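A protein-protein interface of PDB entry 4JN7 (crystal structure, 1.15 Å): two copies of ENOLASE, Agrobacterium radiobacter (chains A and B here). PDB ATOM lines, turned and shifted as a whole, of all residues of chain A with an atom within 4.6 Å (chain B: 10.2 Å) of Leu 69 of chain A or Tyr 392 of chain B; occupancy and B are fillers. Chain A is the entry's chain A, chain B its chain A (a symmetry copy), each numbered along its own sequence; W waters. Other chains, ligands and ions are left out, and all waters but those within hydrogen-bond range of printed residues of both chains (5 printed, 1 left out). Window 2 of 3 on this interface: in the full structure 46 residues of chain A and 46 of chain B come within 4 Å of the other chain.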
ATOM      1  N   PHE A  54       3.433 -19.529  40.248  1.00  0.00           N
ATOM      2  CA  PHE A  54       3.715 -19.322  38.837  1.00  0.00           C
ATOM      3  C   PHE A  54       4.995 -18.530  38.595  1.00  0.00           C
ATOM      4  O   PHE A  54       5.451 -18.425  37.452  1.00  0.00           O
ATOM      5  CB  PHE A  54       2.526 -18.611  38.174  1.00  0.00           C
ATOM      6  CG  PHE A  54       1.212 -19.296  38.432  1.00  0.00           C
ATOM      7  CD1 PHE A  54       0.978 -20.568  37.938  1.00  0.00           C
ATOM      8  CD2 PHE A  54       0.250 -18.718  39.224  1.00  0.00           C
ATOM      9  CE1 PHE A  54      -0.219 -21.222  38.201  1.00  0.00           C
ATOM     10  CE2 PHE A  54      -0.946 -19.369  39.487  1.00  0.00           C
ATOM     11  CZ  PHE A  54      -1.179 -20.611  38.972  1.00  0.00           C
ATOM     12  N   TYR A  65       6.048 -11.348  30.320  1.00  0.00           N
ATOM     13  CA  TYR A  65       5.804 -12.774  30.194  1.00  0.00           C
ATOM     14  C   TYR A  65       5.159 -13.311  31.466  1.00  0.00           C
ATOM     15  O   TYR A  65       4.164 -14.033  31.414  1.00  0.00           O
ATOM     16  CB  TYR A  65       7.148 -13.462  29.952  1.00  0.00           C
ATOM     17  CG  TYR A  65       7.170 -14.975  29.892  1.00  0.00           C
ATOM     18  CD1 TYR A  65       6.675 -15.669  28.800  1.00  0.00           C
ATOM     19  CD2 TYR A  65       7.777 -15.707  30.903  1.00  0.00           C
ATOM     20  CE1 TYR A  65       6.764 -17.057  28.740  1.00  0.00           C
ATOM     21  CE2 TYR A  65       7.865 -17.066  30.852  1.00  0.00           C
ATOM     22  CZ  TYR A  65       7.368 -17.737  29.779  1.00  0.00           C
ATOM     23  OH  TYR A  65       7.473 -19.125  29.766  1.00  0.00           O
ATOM     24  N   LEU A  66       5.746 -12.946  32.605  1.00  0.00           N
ATOM     25  CA  LEU A  66       5.280 -13.457  33.893  1.00  0.00           C
ATOM     26  C   LEU A  66       3.989 -12.765  34.343  1.00  0.00           C
ATOM     27  O   LEU A  66       3.075 -13.416  34.844  1.00  0.00           O
ATOM     28  CB  LEU A  66       6.362 -13.323  34.965  1.00  0.00           C
ATOM     29  CG  LEU A  66       7.596 -14.187  34.700  1.00  0.00           C
ATOM     30  CD1 LEU A  66       8.689 -13.856  35.702  1.00  0.00           C
ATOM     31  CD2 LEU A  66       7.260 -15.675  34.732  1.00  0.00           C
ATOM     32  N   VAL A  67       3.885 -11.454  34.158  1.00  0.00           N
ATOM     33  CA  VAL A  67       2.675 -10.764  34.578  1.00  0.00           C
ATOM     34  C   VAL A  67       1.485 -11.269  33.757  1.00  0.00           C
ATOM     35  O   VAL A  67       0.415 -11.560  34.294  1.00  0.00           O
ATOM     36  CB  VAL A  67       2.813  -9.234  34.483  1.00  0.00           C
ATOM     37  CG1 VAL A  67       1.490  -8.550  34.769  1.00  0.00           C
ATOM     38  CG2 VAL A  67       3.884  -8.724  35.447  1.00  0.00           C
ATOM     39  N   ASN A  68       1.666 -11.425  32.449  1.00  0.00           N
ATOM     40  CA  ASN A  68       0.596 -11.970  31.625  1.00  0.00           C
ATOM     41  C   ASN A  68       0.247 -13.396  32.050  1.00  0.00           C
ATOM     42  O   ASN A  68      -0.909 -13.780  32.010  1.00  0.00           O
ATOM     43  CB  ASN A  68       0.963 -11.930  30.149  1.00  0.00           C
ATOM     44  CG  ASN A  68      -0.145 -12.461  29.274  1.00  0.00           C
ATOM     45  OD1 ASN A  68      -1.263 -11.945  29.269  1.00  0.00           O
ATOM     46  ND2 ASN A  68       0.146 -13.531  28.547  1.00  0.00           N
ATOM     47  N   LEU A  69       1.235 -14.200  32.435  1.00  0.00           N
ATOM     48  CA  LEU A  69       0.926 -15.534  32.937  1.00  0.00           C
ATOM     49  C   LEU A  69      -0.004 -15.437  34.154  1.00  0.00           C
ATOM     50  O   LEU A  69      -0.955 -16.212  34.274  1.00  0.00           O
ATOM     51  CB  LEU A  69       2.200 -16.301  33.297  1.00  0.00           C
ATOM     52  CG  LEU A  69       1.993 -17.687  33.910  1.00  0.00           C
ATOM     53  CD1 LEU A  69       1.194 -18.603  32.983  1.00  0.00           C
ATOM     54  CD2 LEU A  69       3.351 -18.299  34.243  1.00  0.00           C
ATOM     55  N   LEU A  70       0.280 -14.519  35.067  1.00  0.00           N
ATOM     56  CA  LEU A  70      -0.598 -14.329  36.220  1.00  0.00           C
ATOM     57  C   LEU A  70      -2.014 -13.964  35.807  1.00  0.00           C
ATOM     58  O   LEU A  70      -2.984 -14.487  36.358  1.00  0.00           O
ATOM     59  CB  LEU A  70      -0.049 -13.265  37.167  1.00  0.00           C
ATOM     60  CG  LEU A  70       1.356 -13.543  37.722  1.00  0.00           C
ATOM     61  CD1 LEU A  70       1.698 -12.476  38.729  1.00  0.00           C
ATOM     62  CD2 LEU A  70       1.464 -14.945  38.344  1.00  0.00           C
ATOM     63  N   ILE A  71      -2.142 -13.083  34.822  1.00  0.00           N
ATOM     64  CA  ILE A  71      -3.442 -12.712  34.297  1.00  0.00           C
ATOM     65  C   ILE A  71      -4.141 -13.917  33.672  1.00  0.00           C
ATOM     66  O   ILE A  71      -5.337 -14.151  33.899  1.00  0.00           O
ATOM     67  CB  ILE A  71      -3.273 -11.576  33.265  1.00  0.00           C
ATOM     68  CG1 ILE A  71      -2.795 -10.285  33.942  1.00  0.00           C
ATOM     69  CG2 ILE A  71      -4.593 -11.337  32.521  1.00  0.00           C
ATOM     70  CD1 ILE A  71      -2.299  -9.223  32.992  1.00  0.00           C
ATOM     71  N   GLN A  72      -3.424 -14.688  32.866  1.00  0.00           N
ATOM     72  CA  GLN A  72      -4.066 -15.787  32.155  1.00  0.00           C
ATOM     73  C   GLN A  72      -4.427 -16.961  33.071  1.00  0.00           C
ATOM     74  O   GLN A  72      -5.429 -17.648  32.835  1.00  0.00           O
ATOM     75  CB  GLN A  72      -3.214 -16.260  30.969  1.00  0.00           C
ATOM     76  CG  GLN A  72      -2.949 -15.182  29.921  1.00  0.00           C
ATOM     77  CD  GLN A  72      -4.196 -14.470  29.443  1.00  0.00           C
ATOM     78  OE1 GLN A  72      -5.286 -15.041  29.387  1.00  0.00           O
ATOM     79  NE2 GLN A  72      -4.027 -13.223  29.063  1.00  0.00           N
ATOM     80  N   GLN A  73      -3.621 -17.208  34.103  1.00  0.00           N
ATOM     81  CA  GLN A  73      -3.951 -18.248  35.076  1.00  0.00           C
ATOM     82  C   GLN A  73      -5.296 -17.926  35.703  1.00  0.00           C
ATOM     83  O   GLN A  73      -6.095 -18.830  35.990  1.00  0.00           O
ATOM     84  CB  GLN A  73      -2.888 -18.361  36.176  1.00  0.00           C
ATOM     85  CG  GLN A  73      -1.622 -19.102  35.760  1.00  0.00           C
ATOM     86  CD  GLN A  73      -1.828 -20.587  35.490  1.00  0.00           C
ATOM     87  OE1 GLN A  73      -2.786 -21.216  35.956  1.00  0.00           O
ATOM     88  NE2 GLN A  73      -0.919 -21.154  34.733  1.00  0.00           N
ATOM     89  N   HIS B 158      -2.670 -24.301  18.361  1.00  0.00           N
ATOM     90  CA  HIS B 158      -1.503 -23.457  18.098  1.00  0.00           C
ATOM     91  C   HIS B 158      -0.385 -24.199  17.356  1.00  0.00           C
ATOM     92  O   HIS B 158       0.645 -23.600  17.037  1.00  0.00           O
ATOM     93  CB  HIS B 158      -0.970 -22.847  19.409  1.00  0.00           C
ATOM     94  CG  HIS B 158      -1.998 -22.068  20.171  1.00  0.00           C
ATOM     95  ND1 HIS B 158      -2.522 -20.882  19.709  1.00  0.00           N
ATOM     96  CD2 HIS B 158      -2.603 -22.309  21.358  1.00  0.00           C
ATOM     97  CE1 HIS B 158      -3.408 -20.427  20.577  1.00  0.00           C
ATOM     98  NE2 HIS B 158      -3.479 -21.277  21.583  1.00  0.00           N
ATOM     99  N   ALA B 192     -12.762 -19.601  25.337  1.00  0.00           N
ATOM    100  CA  ALA B 192     -12.033 -18.332  25.262  1.00  0.00           C
ATOM    101  C   ALA B 192     -10.601 -18.535  24.765  1.00  0.00           C
ATOM    102  O   ALA B 192      -9.679 -17.860  25.215  1.00  0.00           O
ATOM    103  CB  ALA B 192     -12.072 -17.609  26.604  1.00  0.00           C
ATOM    104  N   GLN B 193     -10.460 -19.466  23.816  1.00  0.00           N
ATOM    105  CA  GLN B 193      -9.176 -19.884  23.243  1.00  0.00           C
ATOM    106  C   GLN B 193      -8.720 -19.026  22.067  1.00  0.00           C
ATOM    107  O   GLN B 193      -7.527 -18.987  21.789  1.00  0.00           O
ATOM    108  CB  GLN B 193      -9.227 -21.356  22.772  1.00  0.00           C
ATOM    109  CG  GLN B 193      -9.261 -22.379  23.891  1.00  0.00           C
ATOM    110  CD  GLN B 193      -8.067 -22.258  24.796  1.00  0.00           C
ATOM    111  OE1 GLN B 193      -6.955 -22.640  24.431  1.00  0.00           O
ATOM    112  NE2 GLN B 193      -8.276 -21.684  25.970  1.00  0.00           N
ATOM    113  N   PHE B 195      -8.125 -15.701  19.725  1.00  0.00           N
ATOM    114  CA  PHE B 195      -7.795 -14.282  19.892  1.00  0.00           C
ATOM    115  C   PHE B 195      -8.607 -13.375  18.965  1.00  0.00           C
ATOM    116  O   PHE B 195      -9.071 -12.313  19.380  1.00  0.00           O
ATOM    117  CB  PHE B 195      -6.300 -14.068  19.631  1.00  0.00           C
ATOM    118  CG  PHE B 195      -5.779 -12.701  20.023  1.00  0.00           C
ATOM    119  CD1 PHE B 195      -5.616 -12.361  21.346  1.00  0.00           C
ATOM    120  CD2 PHE B 195      -5.456 -11.752  19.069  1.00  0.00           C
ATOM    121  CE1 PHE B 195      -5.123 -11.120  21.719  1.00  0.00           C
ATOM    122  CE2 PHE B 195      -4.947 -10.510  19.456  1.00  0.00           C
ATOM    123  CZ  PHE B 195      -4.793 -10.210  20.765  1.00  0.00           C
ATOM    124  N   ARG B 220     -11.873 -13.877  24.128  1.00  0.00           N
ATOM    125  CA  ARG B 220     -11.595 -13.365  25.461  1.00  0.00           C
ATOM    126  C   ARG B 220     -12.648 -12.322  25.863  1.00  0.00           C
ATOM    127  O   ARG B 220     -13.368 -11.777  25.029  1.00  0.00           O
ATOM    128  CB  ARG B 220     -10.190 -12.759  25.506  1.00  0.00           C
ATOM    129  CG  ARG B 220      -9.066 -13.800  25.398  1.00  0.00           C
ATOM    130  CD  ARG B 220      -8.886 -14.647  26.662  1.00  0.00           C
ATOM    131  NE  ARG B 220      -8.539 -13.785  27.785  1.00  0.00           N
ATOM    132  CZ  ARG B 220      -8.784 -14.046  29.070  1.00  0.00           C
ATOM    133  NH1 ARG B 220      -9.339 -15.192  29.435  1.00  0.00           N
ATOM    134  NH2 ARG B 220      -8.488 -13.131  29.970  1.00  0.00           N
ATOM    135  N   GLN B 381      -5.418 -25.354  39.774  1.00  0.00           N
ATOM    136  CA  GLN B 381      -5.045 -24.261  38.882  1.00  0.00           C
ATOM    137  C   GLN B 381      -5.383 -24.612  37.450  1.00  0.00           C
ATOM    138  O   GLN B 381      -5.499 -25.785  37.078  1.00  0.00           O
ATOM    139  CB  GLN B 381      -3.555 -23.938  39.001  1.00  0.00           C
ATOM    140  CG  GLN B 381      -2.641 -25.041  38.499  1.00  0.00           C
ATOM    141  CD  GLN B 381      -1.185 -24.779  38.830  1.00  0.00           C
ATOM    142  OE1 GLN B 381      -0.838 -24.512  39.982  1.00  0.00           O
ATOM    143  NE2 GLN B 381      -0.322 -24.845  37.817  1.00  0.00           N
ATOM    144  N   ARG B 382      -5.541 -23.567  36.646  1.00  0.00           N
ATOM    145  CA  ARG B 382      -5.804 -23.713  35.226  1.00  0.00           C
ATOM    146  C   ARG B 382      -4.548 -24.051  34.470  1.00  0.00           C
ATOM    147  O   ARG B 382      -3.449 -23.778  34.915  1.00  0.00           O
ATOM    148  CB  ARG B 382      -6.386 -22.418  34.663  1.00  0.00           C
ATOM    149  CG  ARG B 382      -7.725 -22.076  35.268  1.00  0.00           C
ATOM    150  CD  ARG B 382      -8.317 -20.762  34.766  1.00  0.00           C
ATOM    151  NE  ARG B 382      -9.574 -20.576  35.473  1.00  0.00           N
ATOM    152  CZ  ARG B 382      -9.670 -20.114  36.716  1.00  0.00           C
ATOM    153  NH1 ARG B 382      -8.598 -19.654  37.365  1.00  0.00           N
ATOM    154  NH2 ARG B 382     -10.844 -20.107  37.312  1.00  0.00           N
ATOM    155  N   ARG B 383      -4.737 -24.642  33.303  1.00  0.00           N
ATOM    156  CA  ARG B 383      -3.647 -24.849  32.375  1.00  0.00           C
ATOM    157  C   ARG B 383      -3.641 -23.746  31.308  1.00  0.00           C
ATOM    158  O   ARG B 383      -4.593 -23.627  30.520  1.00  0.00           O
ATOM    159  CB  ARG B 383      -3.789 -26.219  31.715  1.00  0.00           C
ATOM    160  CG  ARG B 383      -2.736 -26.435  30.667  1.00  0.00           C
ATOM    161  CD  ARG B 383      -2.765 -27.778  29.984  1.00  0.00           C
ATOM    162  NE  ARG B 383      -1.599 -27.798  29.107  1.00  0.00           N
ATOM    163  CZ  ARG B 383      -1.601 -27.433  27.828  1.00  0.00           C
ATOM    164  NH1 ARG B 383      -2.729 -27.082  27.222  1.00  0.00           N
ATOM    165  NH2 ARG B 383      -0.465 -27.455  27.143  1.00  0.00           N
ATOM    166  N   VAL B 384      -2.575 -22.957  31.276  1.00  0.00           N
ATOM    167  CA  VAL B 384      -2.418 -21.939  30.241  1.00  0.00           C
ATOM    168  C   VAL B 384      -1.526 -22.539  29.163  1.00  0.00           C
ATOM    169  O   VAL B 384      -0.344 -22.783  29.399  1.00  0.00           O
ATOM    170  CB  VAL B 384      -1.790 -20.635  30.764  1.00  0.00           C
ATOM    171  CG1 VAL B 384      -1.741 -19.606  29.639  1.00  0.00           C
ATOM    172  CG2 VAL B 384      -2.593 -20.074  31.940  1.00  0.00           C
ATOM    173  N   PRO B 385      -2.095 -22.816  27.989  1.00  0.00           N
ATOM    174  CA  PRO B 385      -1.313 -23.468  26.942  1.00  0.00           C
ATOM    175  C   PRO B 385      -0.234 -22.557  26.372  1.00  0.00           C
ATOM    176  O   PRO B 385      -0.347 -21.326  26.423  1.00  0.00           O
ATOM    177  CB  PRO B 385      -2.361 -23.778  25.872  1.00  0.00           C
ATOM    178  CG  PRO B 385      -3.406 -22.741  26.059  1.00  0.00           C
ATOM    179  CD  PRO B 385      -3.455 -22.481  27.537  1.00  0.00           C
ATOM    180  N   LYS B 386       0.810 -23.169  25.831  1.00  0.00           N
ATOM    181  CA  LYS B 386       1.852 -22.443  25.117  1.00  0.00           C
ATOM    182  C   LYS B 386       1.750 -22.689  23.622  1.00  0.00           C
ATOM    183  O   LYS B 386       1.233 -23.729  23.166  1.00  0.00           O
ATOM    184  CB  LYS B 386       3.242 -22.860  25.594  1.00  0.00           C
ATOM    185  CG  LYS B 386       3.585 -22.429  27.015  1.00  0.00           C
ATOM    186  CD  LYS B 386       5.035 -22.784  27.343  1.00  0.00           C
ATOM    187  CE  LYS B 386       5.549 -22.083  28.599  1.00  0.00           C
ATOM    188  NZ  LYS B 386       6.922 -22.550  28.986  1.00  0.00           N
ATOM    189  N   ARG B 387       2.239 -21.715  22.865  1.00  0.00           N
ATOM    190  CA  ARG B 387       2.431 -21.868  21.436  1.00  0.00           C
ATOM    191  C   ARG B 387       3.803 -22.488  21.205  1.00  0.00           C
ATOM    192  O   ARG B 387       4.648 -22.487  22.108  1.00  0.00           O
ATOM    193  CB  ARG B 387       2.345 -20.506  20.753  1.00  0.00           C
ATOM    194  CG  ARG B 387       1.058 -19.747  21.046  1.00  0.00           C
ATOM    195  CD  ARG B 387       0.938 -18.506  20.192  1.00  0.00           C
ATOM    196  NE  ARG B 387      -0.250 -17.722  20.542  1.00  0.00           N
ATOM    197  CZ  ARG B 387      -0.327 -16.889  21.571  1.00  0.00           C
ATOM    198  NH1 ARG B 387       0.714 -16.715  22.371  1.00  0.00           N
ATOM    199  NH2 ARG B 387      -1.445 -16.234  21.808  1.00  0.00           N
ATOM    200  N   PRO B 388       4.058 -22.994  19.995  1.00  0.00           N
ATOM    201  CA  PRO B 388       5.366 -23.613  19.743  1.00  0.00           C
ATOM    202  C   PRO B 388       6.543 -22.645  19.888  1.00  0.00           C
ATOM    203  O   PRO B 388       7.673 -23.123  20.072  1.00  0.00           O
ATOM    204  CB  PRO B 388       5.239 -24.125  18.306  1.00  0.00           C
ATOM    205  CG  PRO B 388       3.755 -24.374  18.129  1.00  0.00           C
ATOM    206  CD  PRO B 388       3.106 -23.245  18.895  1.00  0.00           C
ATOM    207  N   ASP B 389       6.308 -21.337  19.807  1.00  0.00           N
ATOM    208  CA  ASP B 389       7.384 -20.357  19.994  1.00  0.00           C
ATOM    209  C   ASP B 389       7.694 -20.064  21.460  1.00  0.00           C
ATOM    210  O   ASP B 389       8.577 -19.256  21.747  1.00  0.00           O
ATOM    211  CB  ASP B 389       7.109 -19.050  19.230  1.00  0.00           C
ATOM    212  CG  ASP B 389       5.924 -18.267  19.781  1.00  0.00           C
ATOM    213  OD1 ASP B 389       5.325 -18.679  20.807  1.00  0.00           O
ATOM    214  OD2 ASP B 389       5.568 -17.228  19.161  1.00  0.00           O
ATOM    215  N   GLY B 390       6.984 -20.711  22.385  1.00  0.00           N
ATOM    216  CA  GLY B 390       7.221 -20.516  23.804  1.00  0.00           C
ATOM    217  C   GLY B 390       6.337 -19.483  24.487  1.00  0.00           C
ATOM    218  O   GLY B 390       6.372 -19.345  25.711  1.00  0.00           O
ATOM    219  N   SER B 391       5.548 -18.736  23.720  1.00  0.00           N
ATOM    220  CA  SER B 391       4.631 -17.774  24.313  1.00  0.00           C
ATOM    221  C   SER B 391       3.437 -18.456  24.980  1.00  0.00           C
ATOM    222  O   SER B 391       3.054 -19.586  24.620  1.00  0.00           O
ATOM    223  CB  SER B 391       4.151 -16.771  23.259  1.00  0.00           C
ATOM    224  OG  SER B 391       3.460 -17.408  22.193  1.00  0.00           O
ATOM    225  N   TYR B 392       2.857 -17.787  25.965  1.00  0.00           N
ATOM    226  CA  TYR B 392       1.610 -18.236  26.574  1.00  0.00           C
ATOM    227  C   TYR B 392       0.410 -17.698  25.812  1.00  0.00           C
ATOM    228  O   TYR B 392       0.366 -16.521  25.426  1.00  0.00           O
ATOM    229  CB  TYR B 392       1.511 -17.780  28.030  1.00  0.00           C
ATOM    230  CG  TYR B 392       2.279 -18.650  28.984  1.00  0.00           C
ATOM    231  CD1 TYR B 392       1.881 -19.957  29.227  1.00  0.00           C
ATOM    232  CD2 TYR B 392       3.401 -18.168  29.642  1.00  0.00           C
ATOM    233  CE1 TYR B 392       2.587 -20.756  30.105  1.00  0.00           C
ATOM    234  CE2 TYR B 392       4.115 -18.969  30.521  1.00  0.00           C
ATOM    235  CZ  TYR B 392       3.697 -20.258  30.741  1.00  0.00           C
ATOM    236  OH  TYR B 392       4.394 -21.074  31.617  1.00  0.00           O
ATOM    237  N   ALA B 393      -0.577 -18.567  25.627  1.00  0.00           N
ATOM    238  CA  ALA B 393      -1.849 -18.194  25.013  1.00  0.00           C
ATOM    239  C   ALA B 393      -2.905 -18.032  26.109  1.00  0.00           C
ATOM    240  O   ALA B 393      -2.692 -17.241  27.029  1.00  0.00           O
ATOM    241  CB  ALA B 393      -2.246 -19.198  23.923  1.00  0.00           C
ATOM    242  N   PHE B 394      -4.014 -18.775  26.046  1.00  0.00           N
ATOM    243  CA  PHE B 394      -5.192 -18.476  26.868  1.00  0.00           C
ATOM    244  C   PHE B 394      -5.784 -19.744  27.473  1.00  0.00           C
ATOM    245  O   PHE B 394      -5.890 -20.769  26.790  1.00  0.00           O
ATOM    246  CB  PHE B 394      -6.231 -17.725  26.017  1.00  0.00           C
ATOM    247  CG  PHE B 394      -5.669 -16.503  25.358  1.00  0.00           C
ATOM    248  CD1 PHE B 394      -5.458 -15.353  26.089  1.00  0.00           C
ATOM    249  CD2 PHE B 394      -5.310 -16.502  24.021  1.00  0.00           C
ATOM    250  CE1 PHE B 394      -4.918 -14.227  25.515  1.00  0.00           C
ATOM    251  CE2 PHE B 394      -4.752 -15.365  23.437  1.00  0.00           C
ATOM    252  CZ  PHE B 394      -4.555 -14.238  24.188  1.00  0.00           C
ATOM    253  N   ALA B 395      -6.160 -19.686  28.744  1.00  0.00           N
ATOM    254  CA  ALA B 395      -6.684 -20.865  29.432  1.00  0.00           C
ATOM    255  C   ALA B 395      -8.118 -21.145  29.005  1.00  0.00           C
ATOM    256  O   ALA B 395      -8.928 -20.249  28.822  1.00  0.00           O
ATOM    257  CB  ALA B 395      -6.608 -20.682  30.922  1.00  0.00           C
ATOM    258  OXT ALA B 395      -8.529 -22.292  28.782  1.00  0.00           O
HETATM  259  O   HOH W   1      -6.659 -18.375  39.405  1.00  0.00           O
HETATM  260  O   HOH W   2      -5.177 -20.960  37.940  1.00  0.00           O
HETATM  261  O   HOH W   3      -1.548 -14.739  26.454  1.00  0.00           O
HETATM  262  O   HOH W   4      -0.671 -23.401  33.263  1.00  0.00           O
HETATM  263  O   HOH W   5      -6.529 -17.343  30.244  1.00  0.00           O
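The backbone carbonyl oxygen (O) of Arg 382 of chain B sits close to the side-chain amide oxygen (OE1) of Gln 73 of chain A (2.8 Å).
OD1 of Asn 68 of chain A is in hydrogen-bond range of NE2 of Gln 72 of chain A (3.1 Å).
NE2 of Gln 193 of chain B lies within hydrogen-bond range of OXT of Ala 395 of chain B (2.9 Å).
The side-chain amide nitrogen (NE2) of Gln 193 of chain B is in hydrogen-bond range of the backbone carbonyl oxygen (O) of Phe 394 of chain B, 2.7 Å away.
NH1 of Arg 387 of chain B sits at hydrogen-bond distance from O of Tyr 392 of chain B, at 3.1 Å.
The backbone carbonyl oxygen (O) of Pro 385 of chain B lies within hydrogen-bond range of the backbone NH (N) of Ala 393 of chain B (2.9 Å).
Among the printed residues, pairs that only touch across the chains: Phe 54 of chain A with Gln 381 of chain B, Tyr 65 of chain A with Lys 386 of chain B, Tyr 65 of chain A with Gly 390 of chain B, Tyr 65 of chain A with Tyr 392 of chain B, Leu 69 of chain A with Tyr 392 of chain B, Gln 72 of chain A with Arg 220 of chain B, Gln 72 of chain A with Val 384 of chain B, Gln 72 of chain A with Ala 393 of chain B, Gln 72 of chain A with Phe 394 of chain B, Gln 72 of chain A with Ala 395 of chain B and Gln 73 of chain A with Val 384 of chain B.
Of chain B, only Lys 386 (3.6 Å), Gly 390 (3.8 Å) and Tyr 392 (3.4 Å) come within 4 Å of Tyr 65 of chain A.
No residue of chain B comes within 4 Å of Asn 68 of chain A.
Leu 70 of chain A touches none of the printed residues of chain B.
Of the printed residues of chain B, Gln 72 of chain A touches Arg 220 (3.7 Å), Val 384 (3.8 Å), Ala 393 (3.6 Å), Phe 394 (3.3 Å) and Ala 395 (3.8 Å).
Of chain A, only Tyr 65 and Leu 69 come within 4 Å of Tyr 392 of chain B.
Printed residues of chain A within 4 Å of Phe 394 of chain B: Gln 72.
The nearest residue of chain B that does not touch Leu 69 of chain A is Val 384 of chain B (4.2 Å).
Of the 10 printed residues of chain A, 5 touch a printed residue of chain B.
Printed residues of chain B that touch a printed residue of chain A: Arg 220, Gln 381, Arg 382, Val 384, Lys 386, Gly 390, Tyr 392, Ala 393, Phe 394 and Ala 395.
Hydrophobic or aromatic side chains of chain B within 4 Å of the printed part of chain A: Val 384, Tyr 392, Phe 394 and Ala 395.
Along chain B the printed residues that touch a printed residue of chain A span positions 220 to 395.
Among the printed residues, 12 pairs touch across the chains.
Among the printed residues, no Asp or Glu carboxylate lies within 4 Å of a Lys or Arg side-chain nitrogen of the other chain.
No position is printed for both chains.
Water W4 lies within hydrogen-bond range of the side-chain amide nitrogen of Gln 73 of chain A, the backbone NH of Val 384 of chain B and the backbone carbonyl oxygen of Arg 382 of chain B.
Water W5 lies within hydrogen-bond range of OE1 of Gln 72 of chain A (2.8 Å) and N of Ala 395 of chain B (2.8 Å).
Water W3 lies within hydrogen-bond range of O of Ala 393 of chain B (2.8 Å), O of Tyr 392 of chain B (2.8 Å) and ND2 of Asn 68 of chain A (3.0 Å).
Water W2 lies within hydrogen-bond range of N of Arg 382 of chain B (2.9 Å) and O of Gln 73 of chain A (3.0 Å).
Water W1 bridges NH1 of Arg 382 of chain B (3.1 Å) and O of Gln 73 of chain A (3.5 Å).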
